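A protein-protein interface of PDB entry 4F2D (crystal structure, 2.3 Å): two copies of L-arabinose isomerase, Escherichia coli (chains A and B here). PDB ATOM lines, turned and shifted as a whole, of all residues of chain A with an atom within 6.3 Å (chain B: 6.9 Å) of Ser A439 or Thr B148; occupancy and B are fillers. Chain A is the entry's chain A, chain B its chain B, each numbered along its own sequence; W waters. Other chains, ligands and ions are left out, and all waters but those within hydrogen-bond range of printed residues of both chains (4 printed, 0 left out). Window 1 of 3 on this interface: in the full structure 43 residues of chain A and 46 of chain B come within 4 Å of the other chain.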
ATOM      1  N   TYR A 337      22.188 -13.889  17.943  1.00  0.00           N
ATOM      2  CA  TYR A 337      20.965 -13.851  17.144  1.00  0.00           C
ATOM      3  C   TYR A 337      19.701 -13.733  17.985  1.00  0.00           C
ATOM      4  O   TYR A 337      19.671 -14.079  19.167  1.00  0.00           O
ATOM      5  CB  TYR A 337      20.826 -15.121  16.304  1.00  0.00           C
ATOM      6  CG  TYR A 337      21.889 -15.323  15.255  1.00  0.00           C
ATOM      7  CD1 TYR A 337      22.294 -14.285  14.416  1.00  0.00           C
ATOM      8  CD2 TYR A 337      22.470 -16.568  15.084  1.00  0.00           C
ATOM      9  CE1 TYR A 337      23.268 -14.486  13.455  1.00  0.00           C
ATOM     10  CE2 TYR A 337      23.437 -16.780  14.126  1.00  0.00           C
ATOM     11  CZ  TYR A 337      23.830 -15.738  13.314  1.00  0.00           C
ATOM     12  OH  TYR A 337      24.794 -15.949  12.368  1.00  0.00           O
ATOM     13  N   PHE A 339      16.056 -15.243  17.315  1.00  0.00           N
ATOM     14  CA  PHE A 339      15.201 -16.096  16.483  1.00  0.00           C
ATOM     15  C   PHE A 339      13.720 -15.845  16.764  1.00  0.00           C
ATOM     16  O   PHE A 339      13.233 -16.109  17.865  1.00  0.00           O
ATOM     17  CB  PHE A 339      15.533 -17.577  16.686  1.00  0.00           C
ATOM     18  CG  PHE A 339      16.812 -18.007  16.016  1.00  0.00           C
ATOM     19  CD1 PHE A 339      17.935 -18.323  16.763  1.00  0.00           C
ATOM     20  CD2 PHE A 339      16.890 -18.092  14.631  1.00  0.00           C
ATOM     21  CE1 PHE A 339      19.104 -18.722  16.141  1.00  0.00           C
ATOM     22  CE2 PHE A 339      18.059 -18.487  14.004  1.00  0.00           C
ATOM     23  CZ  PHE A 339      19.169 -18.803  14.761  1.00  0.00           C
ATOM     24  N   ASN A 408      26.791  -8.775   2.099  1.00  0.00           N
ATOM     25  CA  ASN A 408      25.412  -9.053   2.495  1.00  0.00           C
ATOM     26  C   ASN A 408      24.681  -7.737   2.708  1.00  0.00           C
ATOM     27  O   ASN A 408      25.070  -6.937   3.560  1.00  0.00           O
ATOM     28  CB  ASN A 408      25.376  -9.896   3.777  1.00  0.00           C
ATOM     29  CG  ASN A 408      23.963 -10.320   4.186  1.00  0.00           C
ATOM     30  OD1 ASN A 408      23.722 -10.622   5.353  1.00  0.00           O
ATOM     31  ND2 ASN A 408      23.030 -10.352   3.235  1.00  0.00           N
ATOM     32  N   ALA A 431      19.017  -9.450   8.157  1.00  0.00           N
ATOM     33  CA  ALA A 431      19.837  -9.890   7.032  1.00  0.00           C
ATOM     34  C   ALA A 431      18.957 -10.277   5.845  1.00  0.00           C
ATOM     35  O   ALA A 431      18.057 -11.104   5.984  1.00  0.00           O
ATOM     36  CB  ALA A 431      20.705 -11.068   7.447  1.00  0.00           C
ATOM     37  N   ASP A 434      16.672 -13.430   4.200  1.00  0.00           N
ATOM     38  CA  ASP A 434      16.242 -13.818   5.541  1.00  0.00           C
ATOM     39  C   ASP A 434      17.465 -14.362   6.279  1.00  0.00           C
ATOM     40  O   ASP A 434      18.504 -14.588   5.665  1.00  0.00           O
ATOM     41  CB  ASP A 434      15.111 -14.853   5.489  1.00  0.00           C
ATOM     42  CG  ASP A 434      15.431 -16.028   4.590  1.00  0.00           C
ATOM     43  OD1 ASP A 434      16.254 -16.878   4.985  1.00  0.00           O
ATOM     44  OD2 ASP A 434      14.836 -16.123   3.493  1.00  0.00           O
ATOM     45  N   LEU A 435      17.348 -14.572   7.584  1.00  0.00           N
ATOM     46  CA  LEU A 435      18.516 -14.929   8.398  1.00  0.00           C
ATOM     47  C   LEU A 435      19.079 -16.313   8.058  1.00  0.00           C
ATOM     48  O   LEU A 435      20.292 -16.446   7.884  1.00  0.00           O
ATOM     49  CB  LEU A 435      18.233 -14.811   9.900  1.00  0.00           C
ATOM     50  CG  LEU A 435      19.415 -15.130  10.836  1.00  0.00           C
ATOM     51  CD1 LEU A 435      20.705 -14.414  10.438  1.00  0.00           C
ATOM     52  CD2 LEU A 435      19.050 -14.806  12.277  1.00  0.00           C
ATOM     53  N   PRO A 436      18.216 -17.343   7.958  1.00  0.00           N
ATOM     54  CA  PRO A 436      18.744 -18.663   7.607  1.00  0.00           C
ATOM     55  C   PRO A 436      19.491 -18.692   6.278  1.00  0.00           C
ATOM     56  O   PRO A 436      20.609 -19.193   6.218  1.00  0.00           O
ATOM     57  CB  PRO A 436      17.485 -19.535   7.529  1.00  0.00           C
ATOM     58  CG  PRO A 436      16.530 -18.877   8.455  1.00  0.00           C
ATOM     59  CD  PRO A 436      16.782 -17.410   8.299  1.00  0.00           C
ATOM     60  N   THR A 437      18.875 -18.153   5.231  1.00  0.00           N
ATOM     61  CA  THR A 437      19.489 -18.134   3.904  1.00  0.00           C
ATOM     62  C   THR A 437      20.729 -17.237   3.863  1.00  0.00           C
ATOM     63  O   THR A 437      21.734 -17.599   3.257  1.00  0.00           O
ATOM     64  CB  THR A 437      18.482 -17.683   2.825  1.00  0.00           C
ATOM     65  OG1 THR A 437      17.376 -18.599   2.795  1.00  0.00           O
ATOM     66  CG2 THR A 437      19.139 -17.639   1.449  1.00  0.00           C
ATOM     67  N   ALA A 438      20.650 -16.075   4.504  1.00  0.00           N
ATOM     68  CA  ALA A 438      21.771 -15.126   4.528  1.00  0.00           C
ATOM     69  C   ALA A 438      22.978 -15.721   5.246  1.00  0.00           C
ATOM     70  O   ALA A 438      24.099 -15.634   4.756  1.00  0.00           O
ATOM     71  CB  ALA A 438      21.362 -13.815   5.192  1.00  0.00           C
ATOM     72  N   SER A 439      22.734 -16.321   6.409  1.00  0.00           N
ATOM     73  CA  SER A 439      23.794 -16.948   7.198  1.00  0.00           C
ATOM     74  C   SER A 439      24.387 -18.161   6.483  1.00  0.00           C
ATOM     75  O   SER A 439      25.605 -18.342   6.473  1.00  0.00           O
ATOM     76  CB  SER A 439      23.281 -17.357   8.583  1.00  0.00           C
ATOM     77  OG  SER A 439      22.239 -18.321   8.494  1.00  0.00           O
ATOM     78  N   GLU A 440      23.525 -18.981   5.884  1.00  0.00           N
ATOM     79  CA  GLU A 440      23.960 -20.188   5.168  1.00  0.00           C
ATOM     80  C   GLU A 440      24.801 -19.867   3.936  1.00  0.00           C
ATOM     81  O   GLU A 440      25.855 -20.473   3.720  1.00  0.00           O
ATOM     82  CB  GLU A 440      22.755 -21.042   4.761  1.00  0.00           C
ATOM     83  CG  GLU A 440      22.133 -21.807   5.922  1.00  0.00           C
ATOM     84  CD  GLU A 440      20.737 -22.331   5.623  1.00  0.00           C
ATOM     85  OE1 GLU A 440      20.376 -22.482   4.433  1.00  0.00           O
ATOM     86  OE2 GLU A 440      19.992 -22.609   6.588  1.00  0.00           O
ATOM     87  N   ALA A 441      24.327 -18.919   3.131  1.00  0.00           N
ATOM     88  CA  ALA A 441      25.059 -18.462   1.944  1.00  0.00           C
ATOM     89  C   ALA A 441      26.454 -17.944   2.319  1.00  0.00           C
ATOM     90  O   ALA A 441      27.439 -18.227   1.647  1.00  0.00           O
ATOM     91  CB  ALA A 441      24.276 -17.373   1.225  1.00  0.00           C
ATOM     92  N   TRP A 442      26.503 -17.182   3.403  1.00  0.00           N
ATOM     93  CA  TRP A 442      27.741 -16.623   3.939  1.00  0.00           C
ATOM     94  C   TRP A 442      28.682 -17.712   4.378  1.00  0.00           C
ATOM     95  O   TRP A 442      29.879 -17.669   4.075  1.00  0.00           O
ATOM     96  CB  TRP A 442      27.405 -15.727   5.120  1.00  0.00           C
ATOM     97  CG  TRP A 442      28.533 -14.883   5.634  1.00  0.00           C
ATOM     98  CD1 TRP A 442      29.502 -15.237   6.567  1.00  0.00           C
ATOM     99  CD2 TRP A 442      28.821 -13.487   5.291  1.00  0.00           C
ATOM    100  NE1 TRP A 442      30.347 -14.187   6.808  1.00  0.00           N
ATOM    101  CE2 TRP A 442      30.001 -13.111   6.071  1.00  0.00           C
ATOM    102  CE3 TRP A 442      28.247 -12.549   4.441  1.00  0.00           C
ATOM    103  CZ2 TRP A 442      30.565 -11.847   5.987  1.00  0.00           C
ATOM    104  CZ3 TRP A 442      28.827 -11.277   4.363  1.00  0.00           C
ATOM    105  CH2 TRP A 442      29.959 -10.936   5.120  1.00  0.00           C
ATOM    106  N   ILE A 443      28.142 -18.694   5.096  1.00  0.00           N
ATOM    107  CA  ILE A 443      28.925 -19.828   5.598  1.00  0.00           C
ATOM    108  C   ILE A 443      29.419 -20.707   4.446  1.00  0.00           C
ATOM    109  O   ILE A 443      30.590 -21.096   4.416  1.00  0.00           O
ATOM    110  CB  ILE A 443      28.118 -20.665   6.622  1.00  0.00           C
ATOM    111  CG1 ILE A 443      28.010 -19.903   7.948  1.00  0.00           C
ATOM    112  CG2 ILE A 443      28.755 -22.025   6.873  1.00  0.00           C
ATOM    113  CD1 ILE A 443      26.959 -20.453   8.890  1.00  0.00           C
ATOM    114  N   LEU A 444      28.535 -20.991   3.494  1.00  0.00           N
ATOM    115  CA  LEU A 444      28.904 -21.744   2.287  1.00  0.00           C
ATOM    116  C   LEU A 444      30.040 -21.061   1.517  1.00  0.00           C
ATOM    117  O   LEU A 444      30.928 -21.728   0.998  1.00  0.00           O
ATOM    118  CB  LEU A 444      27.693 -21.931   1.364  1.00  0.00           C
ATOM    119  CG  LEU A 444      26.672 -22.989   1.808  1.00  0.00           C
ATOM    120  CD1 LEU A 444      25.369 -22.848   1.029  1.00  0.00           C
ATOM    121  CD2 LEU A 444      27.234 -24.399   1.647  1.00  0.00           C
ATOM    122  N   ILE A 476      24.896 -11.441  -1.413  1.00  0.00           N
ATOM    123  CA  ILE A 476      23.818 -12.027  -0.618  1.00  0.00           C
ATOM    124  C   ILE A 476      22.785 -10.940  -0.329  1.00  0.00           C
ATOM    125  O   ILE A 476      23.039 -10.023   0.451  1.00  0.00           O
ATOM    126  CB  ILE A 476      24.339 -12.623   0.701  1.00  0.00           C
ATOM    127  CG1 ILE A 476      25.434 -13.658   0.423  1.00  0.00           C
ATOM    128  CG2 ILE A 476      23.198 -13.259   1.486  1.00  0.00           C
ATOM    129  CD1 ILE A 476      26.160 -14.118   1.668  1.00  0.00           C
ATOM    130  N   GLN B 102      27.163 -28.462   9.318  1.00  0.00           N
ATOM    131  CA  GLN B 102      27.105 -27.490  10.398  1.00  0.00           C
ATOM    132  C   GLN B 102      25.656 -27.166  10.711  1.00  0.00           C
ATOM    133  O   GLN B 102      24.925 -26.669   9.856  1.00  0.00           O
ATOM    134  CB  GLN B 102      27.835 -26.191  10.065  1.00  0.00           C
ATOM    135  CG  GLN B 102      27.809 -25.224  11.242  1.00  0.00           C
ATOM    136  CD  GLN B 102      28.396 -23.883  10.927  1.00  0.00           C
ATOM    137  OE1 GLN B 102      29.101 -23.728   9.947  1.00  0.00           O
ATOM    138  NE2 GLN B 102      28.135 -22.915  11.778  1.00  0.00           N
ATOM    139  N   PHE B 103      25.258 -27.431  11.949  1.00  0.00           N
ATOM    140  CA  PHE B 103      23.985 -26.942  12.450  1.00  0.00           C
ATOM    141  C   PHE B 103      24.216 -25.580  13.092  1.00  0.00           C
ATOM    142  O   PHE B 103      24.653 -25.475  14.238  1.00  0.00           O
ATOM    143  CB  PHE B 103      23.355 -27.933  13.438  1.00  0.00           C
ATOM    144  CG  PHE B 103      21.939 -27.592  13.836  1.00  0.00           C
ATOM    145  CD1 PHE B 103      21.139 -26.769  13.044  1.00  0.00           C
ATOM    146  CD2 PHE B 103      21.393 -28.124  14.995  1.00  0.00           C
ATOM    147  CE1 PHE B 103      19.845 -26.463  13.417  1.00  0.00           C
ATOM    148  CE2 PHE B 103      20.095 -27.821  15.372  1.00  0.00           C
ATOM    149  CZ  PHE B 103      19.321 -26.992  14.579  1.00  0.00           C
ATOM    150  N   HIS B 104      23.936 -24.535  12.324  1.00  0.00           N
ATOM    151  CA  HIS B 104      24.163 -23.168  12.766  1.00  0.00           C
ATOM    152  C   HIS B 104      23.011 -22.729  13.628  1.00  0.00           C
ATOM    153  O   HIS B 104      22.097 -22.028  13.181  1.00  0.00           O
ATOM    154  CB  HIS B 104      24.348 -22.256  11.567  1.00  0.00           C
ATOM    155  CG  HIS B 104      25.044 -20.963  11.895  1.00  0.00           C
ATOM    156  ND1 HIS B 104      24.538 -19.764  11.568  1.00  0.00           N
ATOM    157  CD2 HIS B 104      26.255 -20.716  12.536  1.00  0.00           C
ATOM    158  CE1 HIS B 104      25.383 -18.801  11.971  1.00  0.00           C
ATOM    159  NE2 HIS B 104      26.428 -19.383  12.569  1.00  0.00           N
ATOM    160  N   THR B 105      23.056 -23.149  14.889  1.00  0.00           N
ATOM    161  CA  THR B 105      21.943 -22.954  15.817  1.00  0.00           C
ATOM    162  C   THR B 105      22.331 -22.112  17.037  1.00  0.00           C
ATOM    163  O   THR B 105      23.423 -21.538  17.090  1.00  0.00           O
ATOM    164  CB  THR B 105      21.366 -24.315  16.264  1.00  0.00           C
ATOM    165  OG1 THR B 105      20.085 -24.117  16.869  1.00  0.00           O
ATOM    166  CG2 THR B 105      22.298 -25.013  17.247  1.00  0.00           C
ATOM    167  N   ARG B 131      30.954 -18.903  11.558  1.00  0.00           N
ATOM    168  CA  ARG B 131      31.472 -18.284  10.338  1.00  0.00           C
ATOM    169  C   ARG B 131      32.971 -18.552  10.167  1.00  0.00           C
ATOM    170  O   ARG B 131      33.441 -18.789   9.053  1.00  0.00           O
ATOM    171  CB  ARG B 131      31.178 -16.781  10.339  1.00  0.00           C
ATOM    172  CG  ARG B 131      29.682 -16.466  10.333  1.00  0.00           C
ATOM    173  CD  ARG B 131      29.315 -14.999  10.405  1.00  0.00           C
ATOM    174  NE  ARG B 131      27.873 -14.873  10.639  1.00  0.00           N
ATOM    175  CZ  ARG B 131      26.978 -14.364   9.792  1.00  0.00           C
ATOM    176  NH1 ARG B 131      27.338 -13.880   8.609  1.00  0.00           N
ATOM    177  NH2 ARG B 131      25.700 -14.330  10.146  1.00  0.00           N
ATOM    178  N   VAL B 146      25.263 -26.872   5.474  1.00  0.00           N
ATOM    179  CA  VAL B 146      24.935 -25.924   6.529  1.00  0.00           C
ATOM    180  C   VAL B 146      23.422 -25.720   6.640  1.00  0.00           C
ATOM    181  O   VAL B 146      22.732 -25.540   5.638  1.00  0.00           O
ATOM    182  CB  VAL B 146      25.652 -24.586   6.310  1.00  0.00           C
ATOM    183  CG1 VAL B 146      25.135 -23.867   5.075  1.00  0.00           C
ATOM    184  CG2 VAL B 146      25.530 -23.713   7.548  1.00  0.00           C
ATOM    185  N   VAL B 147      22.920 -25.781   7.871  1.00  0.00           N
ATOM    186  CA  VAL B 147      21.519 -25.483   8.165  1.00  0.00           C
ATOM    187  C   VAL B 147      21.430 -24.504   9.321  1.00  0.00           C
ATOM    188  O   VAL B 147      21.944 -24.774  10.406  1.00  0.00           O
ATOM    189  CB  VAL B 147      20.722 -26.739   8.547  1.00  0.00           C
ATOM    190  CG1 VAL B 147      19.357 -26.348   9.102  1.00  0.00           C
ATOM    191  CG2 VAL B 147      20.580 -27.666   7.348  1.00  0.00           C
ATOM    192  N   THR B 148      20.767 -23.376   9.083  1.00  0.00           N
ATOM    193  CA  THR B 148      20.582 -22.362  10.108  1.00  0.00           C
ATOM    194  C   THR B 148      19.156 -22.392  10.648  1.00  0.00           C
ATOM    195  O   THR B 148      18.195 -22.473   9.895  1.00  0.00           O
ATOM    196  CB  THR B 148      20.876 -20.942   9.586  1.00  0.00           C
ATOM    197  OG1 THR B 148      22.253 -20.831   9.217  1.00  0.00           O
ATOM    198  CG2 THR B 148      20.566 -19.901  10.665  1.00  0.00           C
ATOM    199  N   GLY B 149      19.044 -22.306  11.967  1.00  0.00           N
ATOM    200  CA  GLY B 149      17.757 -22.218  12.635  1.00  0.00           C
ATOM    201  C   GLY B 149      17.874 -22.585  14.096  1.00  0.00           C
ATOM    202  O   GLY B 149      18.857 -23.200  14.511  1.00  0.00           O
ATOM    203  N   HIS B 150      16.872 -22.200  14.878  1.00  0.00           N
ATOM    204  CA  HIS B 150      16.816 -22.581  16.284  1.00  0.00           C
ATOM    205  C   HIS B 150      16.641 -24.072  16.401  1.00  0.00           C
ATOM    206  O   HIS B 150      15.955 -24.682  15.586  1.00  0.00           O
ATOM    207  CB  HIS B 150      15.694 -21.850  17.004  1.00  0.00           C
ATOM    208  CG  HIS B 150      15.710 -22.061  18.495  1.00  0.00           C
ATOM    209  ND1 HIS B 150      14.789 -22.797  19.132  1.00  0.00           N
ATOM    210  CD2 HIS B 150      16.607 -21.623  19.466  1.00  0.00           C
ATOM    211  CE1 HIS B 150      15.070 -22.822  20.448  1.00  0.00           C
ATOM    212  NE2 HIS B 150      16.182 -22.103  20.651  1.00  0.00           N
ATOM    213  N   ASP B 153      13.299 -25.630  16.054  1.00  0.00           N
ATOM    214  CA  ASP B 153      12.600 -25.334  14.801  1.00  0.00           C
ATOM    215  C   ASP B 153      12.375 -26.617  14.002  1.00  0.00           C
ATOM    216  O   ASP B 153      13.329 -27.288  13.604  1.00  0.00           O
ATOM    217  CB  ASP B 153      13.400 -24.327  13.963  1.00  0.00           C
ATOM    218  CG  ASP B 153      12.617 -23.786  12.770  1.00  0.00           C
ATOM    219  OD1 ASP B 153      11.490 -24.254  12.511  1.00  0.00           O
ATOM    220  OD2 ASP B 153      13.143 -22.885  12.086  1.00  0.00           O
ATOM    221  N   ALA B 156      13.897 -26.784  10.561  1.00  0.00           N
ATOM    222  CA  ALA B 156      15.324 -27.116  10.666  1.00  0.00           C
ATOM    223  C   ALA B 156      15.527 -28.611  10.927  1.00  0.00           C
ATOM    224  O   ALA B 156      16.462 -29.203  10.405  1.00  0.00           O
ATOM    225  CB  ALA B 156      15.996 -26.290  11.752  1.00  0.00           C
ATOM    226  N   ARG B 159      15.240 -30.498   7.598  1.00  0.00           N
ATOM    227  CA  ARG B 159      16.413 -30.325   6.741  1.00  0.00           C
ATOM    228  C   ARG B 159      17.610 -31.108   7.274  1.00  0.00           C
ATOM    229  O   ARG B 159      18.327 -31.746   6.507  1.00  0.00           O
ATOM    230  CB  ARG B 159      16.754 -28.848   6.583  1.00  0.00           C
ATOM    231  CG  ARG B 159      15.710 -28.066   5.809  1.00  0.00           C
ATOM    232  CD  ARG B 159      16.041 -26.582   5.737  1.00  0.00           C
ATOM    233  NE  ARG B 159      17.272 -26.333   4.982  1.00  0.00           N
ATOM    234  CZ  ARG B 159      18.010 -25.221   5.038  1.00  0.00           C
ATOM    235  NH1 ARG B 159      17.678 -24.212   5.836  1.00  0.00           N
ATOM    236  NH2 ARG B 159      19.105 -25.121   4.290  1.00  0.00           N
ATOM    237  N   ILE B 160      17.819 -31.062   8.587  1.00  0.00           N
ATOM    238  CA  ILE B 160      18.888 -31.847   9.222  1.00  0.00           C
ATOM    239  C   ILE B 160      18.652 -33.330   8.972  1.00  0.00           C
ATOM    240  O   ILE B 160      19.556 -34.047   8.550  1.00  0.00           O
ATOM    241  CB  ILE B 160      18.964 -31.635  10.752  1.00  0.00           C
ATOM    242  CG1 ILE B 160      19.329 -30.197  11.115  1.00  0.00           C
ATOM    243  CG2 ILE B 160      19.944 -32.621  11.372  1.00  0.00           C
ATOM    244  CD1 ILE B 160      20.197 -29.502  10.103  1.00  0.00           C
HETATM  245  O   HOH W   1      25.134 -13.326   6.289  1.00  0.00           O
HETATM  246  O   HOH W   2      29.618 -12.111   9.056  1.00  0.00           O
HETATM  247  O   HOH W   3      31.734 -18.506   6.813  1.00  0.00           O
HETATM  248  O   HOH W   4      17.896 -21.710   3.567  1.00  0.00           O
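Water W4 lies within hydrogen-bond range of OE1 of Glu A440, OG1 of Thr A437 and NH1 of Arg B159. Water W3 lies within hydrogen-bond range of the backbone carbonyl oxygen (O) of Arg B131 (2.8 Å) and the backbone carbonyl oxygen (O) of Trp A442 (3.4 Å). Water W2 bridges NH1 of Arg B131 (2.9 Å) and NE1 of Trp A442 (3.1 Å). Water W1 lies within hydrogen-bond range of the backbone carbonyl oxygen (O) of Ala A438, the side-chain amide oxygen (OD1) of Asn A408 and the guanidinium group (NH1) of Arg B131.
OH of Tyr A337 touches CE1 of His B104 (2.9 Å). His B150 touches Phe A339 (N to CE2, 3.99 Å). Thr B148 touches Pro A436 (CB to CA, 3.7 Å). CG1 of Val B146 touches CB of Glu A440, 3.7 Å away. Val B147 touches Glu A440 (CA to OE2, 3.6 Å). CD1 of Trp A442 touches NH1 of Arg B131 (3.3 Å). Gln B102 touches Ile A443. His B104 touches Ile A443 (CG to CD1, 3.6 Å). CG2 of Val B146 touches CG2 of Ile A443 (3.7 Å). CG1 of Val B146 touches CG of Leu A444, at 3.7 Å.
The side-chain hydroxyl (OH) of Tyr A337 sits at hydrogen-bond distance from the guanidinium group (NH2) of Arg B131, at 2.9 Å. The side-chain hydroxyl of Ser A439 sits at hydrogen-bond distance from the side-chain hydroxyl of Thr B148. The side-chain carboxylate (OE2) of Glu A440 lies within salt-bridge range of the guanidinium group (NH1) of Arg B159 (2.9 Å). The backbone NH (N) of Thr B148 lies within hydrogen-bond range of the side-chain carboxylate (OE2) of Glu A440 (2.7 Å).
Of chain B, only Thr B148 comes within 4 Å of Ser A439. Thr B148 touches just these residues of chain A: Pro A436, Ser A439 and Glu A440. Of the printed residues of chain A, His B150 touches Phe A339 (3.99 Å). Of the printed residues of chain A, Arg B131 touches Tyr A337 and Trp A442. Of the printed residues of chain A, Gly B149 touches Phe A339 (3.99 Å). Of the printed residues of chain A, Val B146 touches Glu A440 (3.7 Å), Ile A443 (3.7 Å) and Leu A444 (3.7 Å). Leu A435 touches none of the printed residues of chain B. Thr A437 touches none of the printed residues of chain B.
No position is printed for both chains. Of the 15 pairs that touch across the chains among the printed residues, none has its exchanged pair printed and touching as well.
O of Gln B102 lies within hydrogen-bond range of N of Val B147. O of Pro A436 lies within hydrogen-bond range of OG of Ser A439, 2.9 Å away. O of His B104 lies within hydrogen-bond range of N of Gly B149 (3.3 Å). N of His B104 lies within hydrogen-bond range of O of Val B147, 2.8 Å away. A ring nitrogen (ND1) of His B104 lies within hydrogen-bond range of the side-chain hydroxyl (OG1) of Thr B148 (3.4 Å). O of Gly B149 is in hydrogen-bond range of OG1 of Thr B105 (2.8 Å).
Of the 16 printed residues of chain A, 8 touch a printed residue of chain B. Hydrophobic or aromatic side chains of chain A within 4 Å of the printed part of chain B: Tyr A337, Phe A339, Pro A436, Trp A442, Ile A443 and Leu A444. Along chain A the printed residues that touch a printed residue of chain B span positions 337 to 444. Hydrophobic or aromatic side chains of chain B within 4 Å of the printed part of chain A: His B104 and Val B146. Among the printed residues, 15 pairs touch across the chains. Among the printed residues, Asp or Glu carboxylates within 4 Å of a Lys or Arg side-chain nitrogen of the other chain: Glu A440 with Arg B159 (2.9 Å).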
